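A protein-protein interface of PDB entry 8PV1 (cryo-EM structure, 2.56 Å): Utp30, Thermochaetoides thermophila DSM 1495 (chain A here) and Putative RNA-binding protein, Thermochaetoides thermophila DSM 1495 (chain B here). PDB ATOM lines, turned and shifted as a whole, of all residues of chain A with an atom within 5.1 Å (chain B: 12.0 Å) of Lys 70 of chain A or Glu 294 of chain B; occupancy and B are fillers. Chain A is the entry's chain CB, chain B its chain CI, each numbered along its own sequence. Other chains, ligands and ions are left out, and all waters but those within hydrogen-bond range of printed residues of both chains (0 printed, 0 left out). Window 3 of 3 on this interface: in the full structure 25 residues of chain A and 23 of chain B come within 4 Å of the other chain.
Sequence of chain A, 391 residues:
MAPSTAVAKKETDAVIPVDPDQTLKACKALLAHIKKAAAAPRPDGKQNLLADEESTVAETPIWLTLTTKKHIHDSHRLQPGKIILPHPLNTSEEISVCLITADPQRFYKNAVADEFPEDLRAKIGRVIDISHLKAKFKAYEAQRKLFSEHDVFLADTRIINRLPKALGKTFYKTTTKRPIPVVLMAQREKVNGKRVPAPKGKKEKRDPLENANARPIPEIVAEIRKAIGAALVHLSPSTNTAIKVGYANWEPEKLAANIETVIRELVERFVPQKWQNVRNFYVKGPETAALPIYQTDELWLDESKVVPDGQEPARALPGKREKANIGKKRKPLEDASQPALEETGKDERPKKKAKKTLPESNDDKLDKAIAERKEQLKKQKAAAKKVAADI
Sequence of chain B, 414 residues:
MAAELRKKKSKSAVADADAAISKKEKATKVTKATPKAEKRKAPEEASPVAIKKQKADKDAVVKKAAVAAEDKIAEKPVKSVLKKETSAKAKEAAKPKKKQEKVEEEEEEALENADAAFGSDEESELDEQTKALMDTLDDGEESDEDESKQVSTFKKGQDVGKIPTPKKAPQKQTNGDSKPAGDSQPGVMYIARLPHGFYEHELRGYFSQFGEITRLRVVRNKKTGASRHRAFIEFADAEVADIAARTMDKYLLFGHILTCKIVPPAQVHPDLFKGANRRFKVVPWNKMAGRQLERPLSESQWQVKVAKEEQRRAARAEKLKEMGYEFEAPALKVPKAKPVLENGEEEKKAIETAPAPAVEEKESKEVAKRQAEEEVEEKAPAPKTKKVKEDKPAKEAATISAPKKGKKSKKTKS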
ATOM      1  N   THR A  68      10.574  -8.062  28.802  1.00  0.00           N
ATOM      2  CA  THR A  68      10.617  -7.230  27.611  1.00  0.00           C
ATOM      3  C   THR A  68       9.565  -6.133  27.686  1.00  0.00           C
ATOM      4  O   THR A  68       8.659  -6.159  28.522  1.00  0.00           O
ATOM      5  CB  THR A  68      10.396  -8.061  26.341  1.00  0.00           C
ATOM      6  OG1 THR A  68       9.124  -8.717  26.411  1.00  0.00           O
ATOM      7  CG2 THR A  68      11.491  -9.092  26.178  1.00  0.00           C
ATOM      8  N   LYS A  69       9.703  -5.158  26.787  1.00  0.00           N
ATOM      9  CA  LYS A  69       8.754  -4.052  26.740  1.00  0.00           C
ATOM     10  C   LYS A  69       7.451  -4.472  26.069  1.00  0.00           C
ATOM     11  O   LYS A  69       6.380  -3.946  26.390  1.00  0.00           O
ATOM     12  CB  LYS A  69       9.384  -2.864  26.016  1.00  0.00           C
ATOM     13  CG  LYS A  69      10.630  -2.338  26.700  1.00  0.00           C
ATOM     14  CD  LYS A  69      11.330  -1.292  25.858  1.00  0.00           C
ATOM     15  CE  LYS A  69      12.656  -0.903  26.481  1.00  0.00           C
ATOM     16  NZ  LYS A  69      13.402   0.081  25.646  1.00  0.00           N
ATOM     17  N   LYS A  70       7.527  -5.402  25.124  1.00  0.00           N
ATOM     18  CA  LYS A  70       6.371  -5.911  24.400  1.00  0.00           C
ATOM     19  C   LYS A  70       6.256  -7.421  24.590  1.00  0.00           C
ATOM     20  O   LYS A  70       7.038  -8.047  25.311  1.00  0.00           O
ATOM     21  CB  LYS A  70       6.476  -5.556  22.916  1.00  0.00           C
ATOM     22  CG  LYS A  70       7.595  -6.288  22.195  1.00  0.00           C
ATOM     23  CD  LYS A  70       7.744  -5.846  20.749  1.00  0.00           C
ATOM     24  CE  LYS A  70       6.689  -6.479  19.858  1.00  0.00           C
ATOM     25  NZ  LYS A  70       6.817  -6.025  18.447  1.00  0.00           N
ATOM     26  N   HIS A  71       5.258  -8.006  23.932  1.00  0.00           N
ATOM     27  CA  HIS A  71       5.162  -9.456  23.859  1.00  0.00           C
ATOM     28  C   HIS A  71       6.252  -9.991  22.940  1.00  0.00           C
ATOM     29  O   HIS A  71       6.465  -9.464  21.845  1.00  0.00           O
ATOM     30  CB  HIS A  71       3.783  -9.880  23.353  1.00  0.00           C
ATOM     31  CG  HIS A  71       2.688  -9.708  24.358  1.00  0.00           C
ATOM     32  ND1 HIS A  71       1.381 -10.063  24.102  1.00  0.00           N
ATOM     33  CD2 HIS A  71       2.704  -9.223  25.622  1.00  0.00           C
ATOM     34  CE1 HIS A  71       0.640  -9.802  25.163  1.00  0.00           C
ATOM     35  NE2 HIS A  71       1.419  -9.291  26.100  1.00  0.00           N
ATOM     36  N   ILE A  72       6.949 -11.035  23.392  1.00  0.00           N
ATOM     37  CA  ILE A  72       8.070 -11.563  22.621  1.00  0.00           C
ATOM     38  C   ILE A  72       7.579 -12.295  21.375  1.00  0.00           C
ATOM     39  O   ILE A  72       8.300 -12.387  20.375  1.00  0.00           O
ATOM     40  CB  ILE A  72       8.952 -12.453  23.524  1.00  0.00           C
ATOM     41  CG1 ILE A  72      10.287 -12.780  22.848  1.00  0.00           C
ATOM     42  CG2 ILE A  72       8.222 -13.723  23.940  1.00  0.00           C
ATOM     43  CD1 ILE A  72      11.254 -13.512  23.745  1.00  0.00           C
ATOM     44  N   SER A 238       3.905 -12.837  25.810  1.00  0.00           N
ATOM     45  CA  SER A 238       4.135 -12.366  27.165  1.00  0.00           C
ATOM     46  C   SER A 238       5.372 -11.487  27.191  1.00  0.00           C
ATOM     47  O   SER A 238       6.209 -11.519  26.285  1.00  0.00           O
ATOM     48  CB  SER A 238       4.309 -13.528  28.139  1.00  0.00           C
ATOM     49  OG  SER A 238       5.551 -14.178  27.939  1.00  0.00           O
ATOM     50  N   THR A 239       5.479 -10.698  28.255  1.00  0.00           N
ATOM     51  CA  THR A 239       6.676  -9.925  28.536  1.00  0.00           C
ATOM     52  C   THR A 239       7.704 -10.713  29.334  1.00  0.00           C
ATOM     53  O   THR A 239       8.817 -10.221  29.531  1.00  0.00           O
ATOM     54  CB  THR A 239       6.312  -8.645  29.291  1.00  0.00           C
ATOM     55  OG1 THR A 239       5.469  -8.969  30.404  1.00  0.00           O
ATOM     56  CG2 THR A 239       5.578  -7.683  28.375  1.00  0.00           C
ATOM     57  N   PRO A 272      12.707 -10.076  19.233  1.00  0.00           N
ATOM     58  CA  PRO A 272      12.561  -9.061  18.187  1.00  0.00           C
ATOM     59  C   PRO A 272      13.019  -7.700  18.682  1.00  0.00           C
ATOM     60  O   PRO A 272      12.960  -7.402  19.878  1.00  0.00           O
ATOM     61  CB  PRO A 272      11.058  -9.072  17.891  1.00  0.00           C
ATOM     62  CG  PRO A 272      10.440  -9.536  19.166  1.00  0.00           C
ATOM     63  CD  PRO A 272      11.404 -10.537  19.742  1.00  0.00           C
ATOM     64  N   ASN A 277      14.101  -3.890  22.815  1.00  0.00           N
ATOM     65  CA  ASN A 277      12.957  -4.528  23.456  1.00  0.00           C
ATOM     66  C   ASN A 277      13.291  -4.986  24.871  1.00  0.00           C
ATOM     67  O   ASN A 277      12.390  -5.155  25.699  1.00  0.00           O
ATOM     68  CB  ASN A 277      12.487  -5.713  22.615  1.00  0.00           C
ATOM     69  CG  ASN A 277      11.101  -6.176  22.985  1.00  0.00           C
ATOM     70  OD1 ASN A 277      10.369  -5.484  23.693  1.00  0.00           O
ATOM     71  ND2 ASN A 277      10.732  -7.362  22.516  1.00  0.00           N
ATOM     72  N   LEU A 301      10.261   1.414  23.301  1.00  0.00           N
ATOM     73  CA  LEU A 301      10.902   0.704  22.198  1.00  0.00           C
ATOM     74  C   LEU A 301      11.715   1.660  21.334  1.00  0.00           C
ATOM     75  O   LEU A 301      12.866   1.372  20.982  1.00  0.00           O
ATOM     76  CB  LEU A 301       9.852  -0.022  21.357  1.00  0.00           C
ATOM     77  CG  LEU A 301       9.103  -1.167  22.042  1.00  0.00           C
ATOM     78  CD1 LEU A 301       7.999  -1.704  21.144  1.00  0.00           C
ATOM     79  CD2 LEU A 301      10.073  -2.273  22.417  1.00  0.00           C
ATOM     80  N   LYS A 305       7.027   5.805  20.255  1.00  0.00           N
ATOM     81  CA  LYS A 305       6.121   5.619  21.385  1.00  0.00           C
ATOM     82  C   LYS A 305       5.919   6.922  22.148  1.00  0.00           C
ATOM     83  O   LYS A 305       4.840   7.167  22.701  1.00  0.00           O
ATOM     84  CB  LYS A 305       6.656   4.528  22.311  1.00  0.00           C
ATOM     85  CG  LYS A 305       6.787   3.167  21.649  1.00  0.00           C
ATOM     86  CD  LYS A 305       5.425   2.599  21.285  1.00  0.00           C
ATOM     87  CE  LYS A 305       5.534   1.167  20.787  1.00  0.00           C
ATOM     88  NZ  LYS A 305       6.174   1.092  19.445  1.00  0.00           N
ATOM     89  N   TRP B 285      -8.107 -11.109  25.745  1.00  0.00           N
ATOM     90  CA  TRP B 285      -7.514 -10.229  26.749  1.00  0.00           C
ATOM     91  C   TRP B 285      -6.001 -10.141  26.586  1.00  0.00           C
ATOM     92  O   TRP B 285      -5.400  -9.081  26.798  1.00  0.00           O
ATOM     93  CB  TRP B 285      -7.873 -10.718  28.152  1.00  0.00           C
ATOM     94  CG  TRP B 285      -9.295 -11.163  28.303  1.00  0.00           C
ATOM     95  CD1 TRP B 285      -9.760 -12.443  28.255  1.00  0.00           C
ATOM     96  CD2 TRP B 285     -10.434 -10.333  28.566  1.00  0.00           C
ATOM     97  NE1 TRP B 285     -11.118 -12.462  28.450  1.00  0.00           N
ATOM     98  CE2 TRP B 285     -11.556 -11.179  28.646  1.00  0.00           C
ATOM     99  CE3 TRP B 285     -10.614  -8.956  28.733  1.00  0.00           C
ATOM    100  CZ2 TRP B 285     -12.839 -10.697  28.885  1.00  0.00           C
ATOM    101  CZ3 TRP B 285     -11.891  -8.479  28.970  1.00  0.00           C
ATOM    102  CH2 TRP B 285     -12.986  -9.348  29.044  1.00  0.00           C
ATOM    103  N   ASN B 286      -5.369 -11.254  26.211  1.00  0.00           N
ATOM    104  CA  ASN B 286      -3.927 -11.266  25.991  1.00  0.00           C
ATOM    105  C   ASN B 286      -3.548 -10.393  24.795  1.00  0.00           C
ATOM    106  O   ASN B 286      -2.549  -9.659  24.834  1.00  0.00           O
ATOM    107  CB  ASN B 286      -3.472 -12.714  25.805  1.00  0.00           C
ATOM    108  CG  ASN B 286      -1.974 -12.868  25.775  1.00  0.00           C
ATOM    109  OD1 ASN B 286      -1.260 -12.111  26.424  1.00  0.00           O
ATOM    110  ND2 ASN B 286      -1.483 -13.821  24.992  1.00  0.00           N
ATOM    111  N   LYS B 287      -4.358 -10.435  23.732  1.00  0.00           N
ATOM    112  CA  LYS B 287      -4.131  -9.557  22.588  1.00  0.00           C
ATOM    113  C   LYS B 287      -4.416  -8.097  22.930  1.00  0.00           C
ATOM    114  O   LYS B 287      -3.725  -7.199  22.435  1.00  0.00           O
ATOM    115  CB  LYS B 287      -4.971 -10.016  21.395  1.00  0.00           C
ATOM    116  CG  LYS B 287      -4.709 -11.460  20.945  1.00  0.00           C
ATOM    117  CD  LYS B 287      -3.271 -11.682  20.475  1.00  0.00           C
ATOM    118  CE  LYS B 287      -3.031 -11.060  19.106  1.00  0.00           C
ATOM    119  NZ  LYS B 287      -3.822 -11.729  18.031  1.00  0.00           N
ATOM    120  N   MET B 288      -5.419  -7.835  23.783  1.00  0.00           N
ATOM    121  CA  MET B 288      -5.616  -6.473  24.282  1.00  0.00           C
ATOM    122  C   MET B 288      -4.400  -5.975  25.041  1.00  0.00           C
ATOM    123  O   MET B 288      -4.011  -4.810  24.912  1.00  0.00           O
ATOM    124  CB  MET B 288      -6.835  -6.361  25.198  1.00  0.00           C
ATOM    125  CG  MET B 288      -8.185  -6.538  24.567  1.00  0.00           C
ATOM    126  SD  MET B 288      -9.418  -6.348  25.870  1.00  0.00           S
ATOM    127  CE  MET B 288     -10.925  -6.656  24.966  1.00  0.00           C
ATOM    128  N   ALA B 289      -3.810  -6.840  25.864  1.00  0.00           N
ATOM    129  CA  ALA B 289      -2.636  -6.448  26.634  1.00  0.00           C
ATOM    130  C   ALA B 289      -1.460  -6.147  25.718  1.00  0.00           C
ATOM    131  O   ALA B 289      -0.746  -5.151  25.908  1.00  0.00           O
ATOM    132  CB  ALA B 289      -2.282  -7.547  27.631  1.00  0.00           C
ATOM    133  N   GLY B 290      -1.260  -6.989  24.701  1.00  0.00           N
ATOM    134  CA  GLY B 290      -0.199  -6.729  23.742  1.00  0.00           C
ATOM    135  C   GLY B 290      -0.392  -5.419  23.007  1.00  0.00           C
ATOM    136  O   GLY B 290       0.541  -4.623  22.877  1.00  0.00           O
ATOM    137  N   ARG B 291      -1.628  -5.140  22.587  1.00  0.00           N
ATOM    138  CA  ARG B 291      -1.904  -3.895  21.876  1.00  0.00           C
ATOM    139  C   ARG B 291      -1.757  -2.677  22.779  1.00  0.00           C
ATOM    140  O   ARG B 291      -1.294  -1.624  22.328  1.00  0.00           O
ATOM    141  CB  ARG B 291      -3.296  -3.948  21.258  1.00  0.00           C
ATOM    142  CG  ARG B 291      -3.384  -4.967  20.152  1.00  0.00           C
ATOM    143  CD  ARG B 291      -4.748  -5.004  19.512  1.00  0.00           C
ATOM    144  NE  ARG B 291      -4.825  -6.057  18.509  1.00  0.00           N
ATOM    145  CZ  ARG B 291      -4.504  -5.901  17.231  1.00  0.00           C
ATOM    146  NH1 ARG B 291      -4.117  -4.729  16.754  1.00  0.00           N
ATOM    147  NH2 ARG B 291      -4.577  -6.945  16.411  1.00  0.00           N
ATOM    148  N   GLN B 292      -2.143  -2.787  24.053  1.00  0.00           N
ATOM    149  CA  GLN B 292      -2.044  -1.612  24.912  1.00  0.00           C
ATOM    150  C   GLN B 292      -0.603  -1.340  25.321  1.00  0.00           C
ATOM    151  O   GLN B 292      -0.261  -0.195  25.634  1.00  0.00           O
ATOM    152  CB  GLN B 292      -2.934  -1.739  26.149  1.00  0.00           C
ATOM    153  CG  GLN B 292      -2.544  -2.806  27.141  1.00  0.00           C
ATOM    154  CD  GLN B 292      -3.510  -2.887  28.302  1.00  0.00           C
ATOM    155  OE1 GLN B 292      -4.457  -2.105  28.391  1.00  0.00           O
ATOM    156  NE2 GLN B 292      -3.269  -3.825  29.209  1.00  0.00           N
ATOM    157  N   LEU B 293       0.259  -2.361  25.334  1.00  0.00           N
ATOM    158  CA  LEU B 293       1.682  -2.040  25.441  1.00  0.00           C
ATOM    159  C   LEU B 293       2.273  -1.594  24.104  1.00  0.00           C
ATOM    160  O   LEU B 293       3.349  -0.987  24.085  1.00  0.00           O
ATOM    161  CB  LEU B 293       2.488  -3.190  26.057  1.00  0.00           C
ATOM    162  CG  LEU B 293       2.414  -3.346  27.593  1.00  0.00           C
ATOM    163  CD1 LEU B 293       1.095  -3.863  28.161  1.00  0.00           C
ATOM    164  CD2 LEU B 293       3.586  -4.173  28.120  1.00  0.00           C
ATOM    165  N   GLU B 294       1.604  -1.880  22.986  1.00  0.00           N
ATOM    166  CA  GLU B 294       2.008  -1.304  21.703  1.00  0.00           C
ATOM    167  C   GLU B 294       1.477   0.103  21.448  1.00  0.00           C
ATOM    168  O   GLU B 294       1.894   0.721  20.467  1.00  0.00           O
ATOM    169  CB  GLU B 294       1.589  -2.203  20.534  1.00  0.00           C
ATOM    170  CG  GLU B 294       2.294  -3.536  20.471  1.00  0.00           C
ATOM    171  CD  GLU B 294       3.769  -3.392  20.173  1.00  0.00           C
ATOM    172  OE1 GLU B 294       4.154  -2.445  19.457  1.00  0.00           O
ATOM    173  OE2 GLU B 294       4.550  -4.224  20.665  1.00  0.00           O
ATOM    174  N   ARG B 295       0.556   0.621  22.278  1.00  0.00           N
ATOM    175  CA  ARG B 295       0.045   1.967  22.008  1.00  0.00           C
ATOM    176  C   ARG B 295       1.064   3.037  22.406  1.00  0.00           C
ATOM    177  O   ARG B 295       1.717   2.913  23.444  1.00  0.00           O
ATOM    178  CB  ARG B 295      -1.264   2.227  22.755  1.00  0.00           C
ATOM    179  CG  ARG B 295      -2.446   1.396  22.305  1.00  0.00           C
ATOM    180  CD  ARG B 295      -3.670   1.703  23.150  1.00  0.00           C
ATOM    181  NE  ARG B 295      -4.123   3.079  22.977  1.00  0.00           N
ATOM    182  CZ  ARG B 295      -4.970   3.472  22.036  1.00  0.00           C
ATOM    183  NH1 ARG B 295      -5.473   2.620  21.159  1.00  0.00           N
ATOM    184  NH2 ARG B 295      -5.322   4.754  21.975  1.00  0.00           N
ATOM    185  N   PRO B 296       1.244   4.071  21.579  1.00  0.00           N
ATOM    186  CA  PRO B 296       1.919   5.281  22.055  1.00  0.00           C
ATOM    187  C   PRO B 296       1.179   5.903  23.229  1.00  0.00           C
ATOM    188  O   PRO B 296      -0.053   5.890  23.289  1.00  0.00           O
ATOM    189  CB  PRO B 296       1.859   6.206  20.834  1.00  0.00           C
ATOM    190  CG  PRO B 296       1.706   5.273  19.633  1.00  0.00           C
ATOM    191  CD  PRO B 296       1.578   3.863  20.162  1.00  0.00           C
ATOM    192  N   LEU B 297       1.943   6.455  24.168  1.00  0.00           N
ATOM    193  CA  LEU B 297       1.383   7.227  25.266  1.00  0.00           C
ATOM    194  C   LEU B 297       2.097   8.569  25.339  1.00  0.00           C
ATOM    195  O   LEU B 297       3.222   8.728  24.860  1.00  0.00           O
ATOM    196  CB  LEU B 297       1.492   6.503  26.620  1.00  0.00           C
ATOM    197  CG  LEU B 297       0.468   5.443  27.063  1.00  0.00           C
ATOM    198  CD1 LEU B 297      -0.930   6.041  27.225  1.00  0.00           C
ATOM    199  CD2 LEU B 297       0.438   4.202  26.180  1.00  0.00           C
ATOM    200  N   SER B 298       1.421   9.542  25.942  1.00  0.00           N
ATOM    201  CA  SER B 298       1.950  10.892  26.033  1.00  0.00           C
ATOM    202  C   SER B 298       2.900  11.038  27.217  1.00  0.00           C
ATOM    203  O   SER B 298       3.008  10.156  28.081  1.00  0.00           O
ATOM    204  CB  SER B 298       0.815  11.911  26.142  1.00  0.00           C
ATOM    205  OG  SER B 298      -0.074  11.798  25.044  1.00  0.00           O
ATOM    206  N   GLN B 301       1.803  10.716  31.238  1.00  0.00           N
ATOM    207  CA  GLN B 301       1.635   9.365  31.753  1.00  0.00           C
ATOM    208  C   GLN B 301       2.899   8.527  31.585  1.00  0.00           C
ATOM    209  O   GLN B 301       3.093   7.561  32.335  1.00  0.00           O
ATOM    210  CB  GLN B 301       0.405   8.698  31.127  1.00  0.00           C
ATOM    211  CG  GLN B 301       0.383   8.536  29.623  1.00  0.00           C
ATOM    212  CD  GLN B 301      -0.247   9.739  28.937  1.00  0.00           C
ATOM    213  OE1 GLN B 301      -0.257  10.844  29.480  1.00  0.00           O
ATOM    214  NE2 GLN B 301      -0.857   9.505  27.783  1.00  0.00           N
ATOM    215  N   TRP B 302       3.806   8.906  30.675  1.00  0.00           N
ATOM    216  CA  TRP B 302       5.135   8.295  30.724  1.00  0.00           C
ATOM    217  C   TRP B 302       5.897   8.696  31.987  1.00  0.00           C
ATOM    218  O   TRP B 302       6.635   7.880  32.552  1.00  0.00           O
ATOM    219  CB  TRP B 302       5.963   8.613  29.478  1.00  0.00           C
ATOM    220  CG  TRP B 302       5.711   7.672  28.345  1.00  0.00           C
ATOM    221  CD1 TRP B 302       4.767   7.777  27.373  1.00  0.00           C
ATOM    222  CD2 TRP B 302       6.367   6.418  28.131  1.00  0.00           C
ATOM    223  NE1 TRP B 302       4.833   6.694  26.529  1.00  0.00           N
ATOM    224  CE2 TRP B 302       5.802   5.839  26.982  1.00  0.00           C
ATOM    225  CE3 TRP B 302       7.393   5.738  28.794  1.00  0.00           C
ATOM    226  CZ2 TRP B 302       6.226   4.613  26.478  1.00  0.00           C
ATOM    227  CZ3 TRP B 302       7.810   4.519  28.294  1.00  0.00           C
ATOM    228  CH2 TRP B 302       7.230   3.971  27.147  1.00  0.00           C
ATOM    229  N   LYS B 305       4.466   6.449  34.671  1.00  0.00           N
ATOM    230  CA  LYS B 305       5.004   5.095  34.553  1.00  0.00           C
ATOM    231  C   LYS B 305       6.439   5.005  35.047  1.00  0.00           C
ATOM    232  O   LYS B 305       6.784   4.091  35.814  1.00  0.00           O
ATOM    233  CB  LYS B 305       4.940   4.631  33.101  1.00  0.00           C
ATOM    234  CG  LYS B 305       3.558   4.335  32.583  1.00  0.00           C
ATOM    235  CD  LYS B 305       3.659   3.843  31.155  1.00  0.00           C
ATOM    236  CE  LYS B 305       4.281   2.455  31.095  1.00  0.00           C
ATOM    237  NZ  LYS B 305       4.300   1.913  29.706  1.00  0.00           N
ATOM    238  N   ARG B 312       9.278   0.993  42.341  1.00  0.00           N
ATOM    239  CA  ARG B 312       9.347  -0.465  42.228  1.00  0.00           C
ATOM    240  C   ARG B 312      10.786  -0.962  42.369  1.00  0.00           C
ATOM    241  O   ARG B 312      11.057  -1.934  43.090  1.00  0.00           O
ATOM    242  CB  ARG B 312       8.734  -0.926  40.907  1.00  0.00           C
ATOM    243  CG  ARG B 312       8.899  -2.415  40.660  1.00  0.00           C
ATOM    244  CD  ARG B 312       7.939  -2.922  39.605  1.00  0.00           C
ATOM    245  NE  ARG B 312       8.020  -2.173  38.357  1.00  0.00           N
ATOM    246  CZ  ARG B 312       7.254  -2.408  37.301  1.00  0.00           C
ATOM    247  NH1 ARG B 312       6.344  -3.369  37.307  1.00  0.00           N
ATOM    248  NH2 ARG B 312       7.400  -1.660  36.213  1.00  0.00           N
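NZ of Lys 70 of chain A lies within salt-bridge range of OE2 of Glu 294 of chain B (3.6 Å).
The backbone carbonyl oxygen (O) of Lys 305 of chain A is in hydrogen-bond range of the backbone NH (N) of Leu 297 of chain B, 3.3 Å away.
The backbone carbonyl oxygen (O) of Lys 70 of chain A lies within hydrogen-bond range of the side-chain hydroxyl (OG1) of Thr 68 of chain A (2.5 Å).
The backbone NH (N) of Lys 69 of chain A is in hydrogen-bond range of the backbone carbonyl oxygen (O) of Asn 277 of chain A (2.9 Å).
The backbone NH (N) of Lys 70 of chain A lies within hydrogen-bond range of the side-chain amide oxygen (OD1) of Asn 277 of chain A (3.2 Å).
O of Leu 297 of chain B is in hydrogen-bond range of NE1 of Trp 302 of chain B, at 3.1 Å.
Among the printed residues, pairs that only touch across the chains: Lys 69 of chain A with Leu 293 of chain B (3.3 Å), His 71 of chain A with Asn 286 of chain B (3.2 Å), His 71 of chain A with Gly 290 of chain B (3.4 Å), Lys 305 of chain A with Glu 294 of chain B (3.7 Å), Lys 305 of chain A with Pro 296 of chain B (3.5 Å) and Lys 305 of chain A with Trp 302 of chain B (3.9 Å).
No residue of chain B comes within 4 Å of Thr 68 of chain A.
Of the printed residues of chain B, Lys 69 of chain A touches Leu 293.
His 71 of chain A touches just these residues of chain B: Asn 286 and Gly 290.
No residue of chain B comes within 4 Å of Ser 238 of chain A.
No residue of chain B comes within 4 Å of Thr 239 of chain A.
No residue of chain B comes within 4 Å of Pro 272 of chain A.
No residue of chain B comes within 4 Å of Asn 277 of chain A.
Of chain B, only Glu 294, Pro 296, Leu 297 and Trp 302 come within 4 Å of Lys 305 of chain A.
Of the printed residues of chain A, Asn 286 of chain B touches His 71 (3.2 Å).
Lys 287 of chain B touches none of the printed residues of chain A.
Met 288 of chain B touches none of the printed residues of chain A.
Glu 294 of chain B touches two residues of chain A.
Of the printed residues of chain A, Trp 302 of chain B touches Lys 305.
The nearest residue of chain B that does not touch Lys 70 of chain A is Leu 293 of chain B (5.0 Å).
The nearest printed residue of chain A that does not touch Leu 297 of chain B is Leu 301 of chain A (9.8 Å).
Along chain B the printed residues that touch a printed residue of chain A span positions 286 to 302.
Of the 11 printed residues of chain A, 4 touch a printed residue of chain B.
Hydrophobic or aromatic side chains of chain A that line the printed part of chain B: His 71.
Among the printed residues, 8 pairs touch across the chains.
Among the printed residues, Asp or Glu carboxylates within 4 Å of a Lys or Arg side-chain nitrogen of the other chain: Lys 70 of chain A with Glu 294 of chain B.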
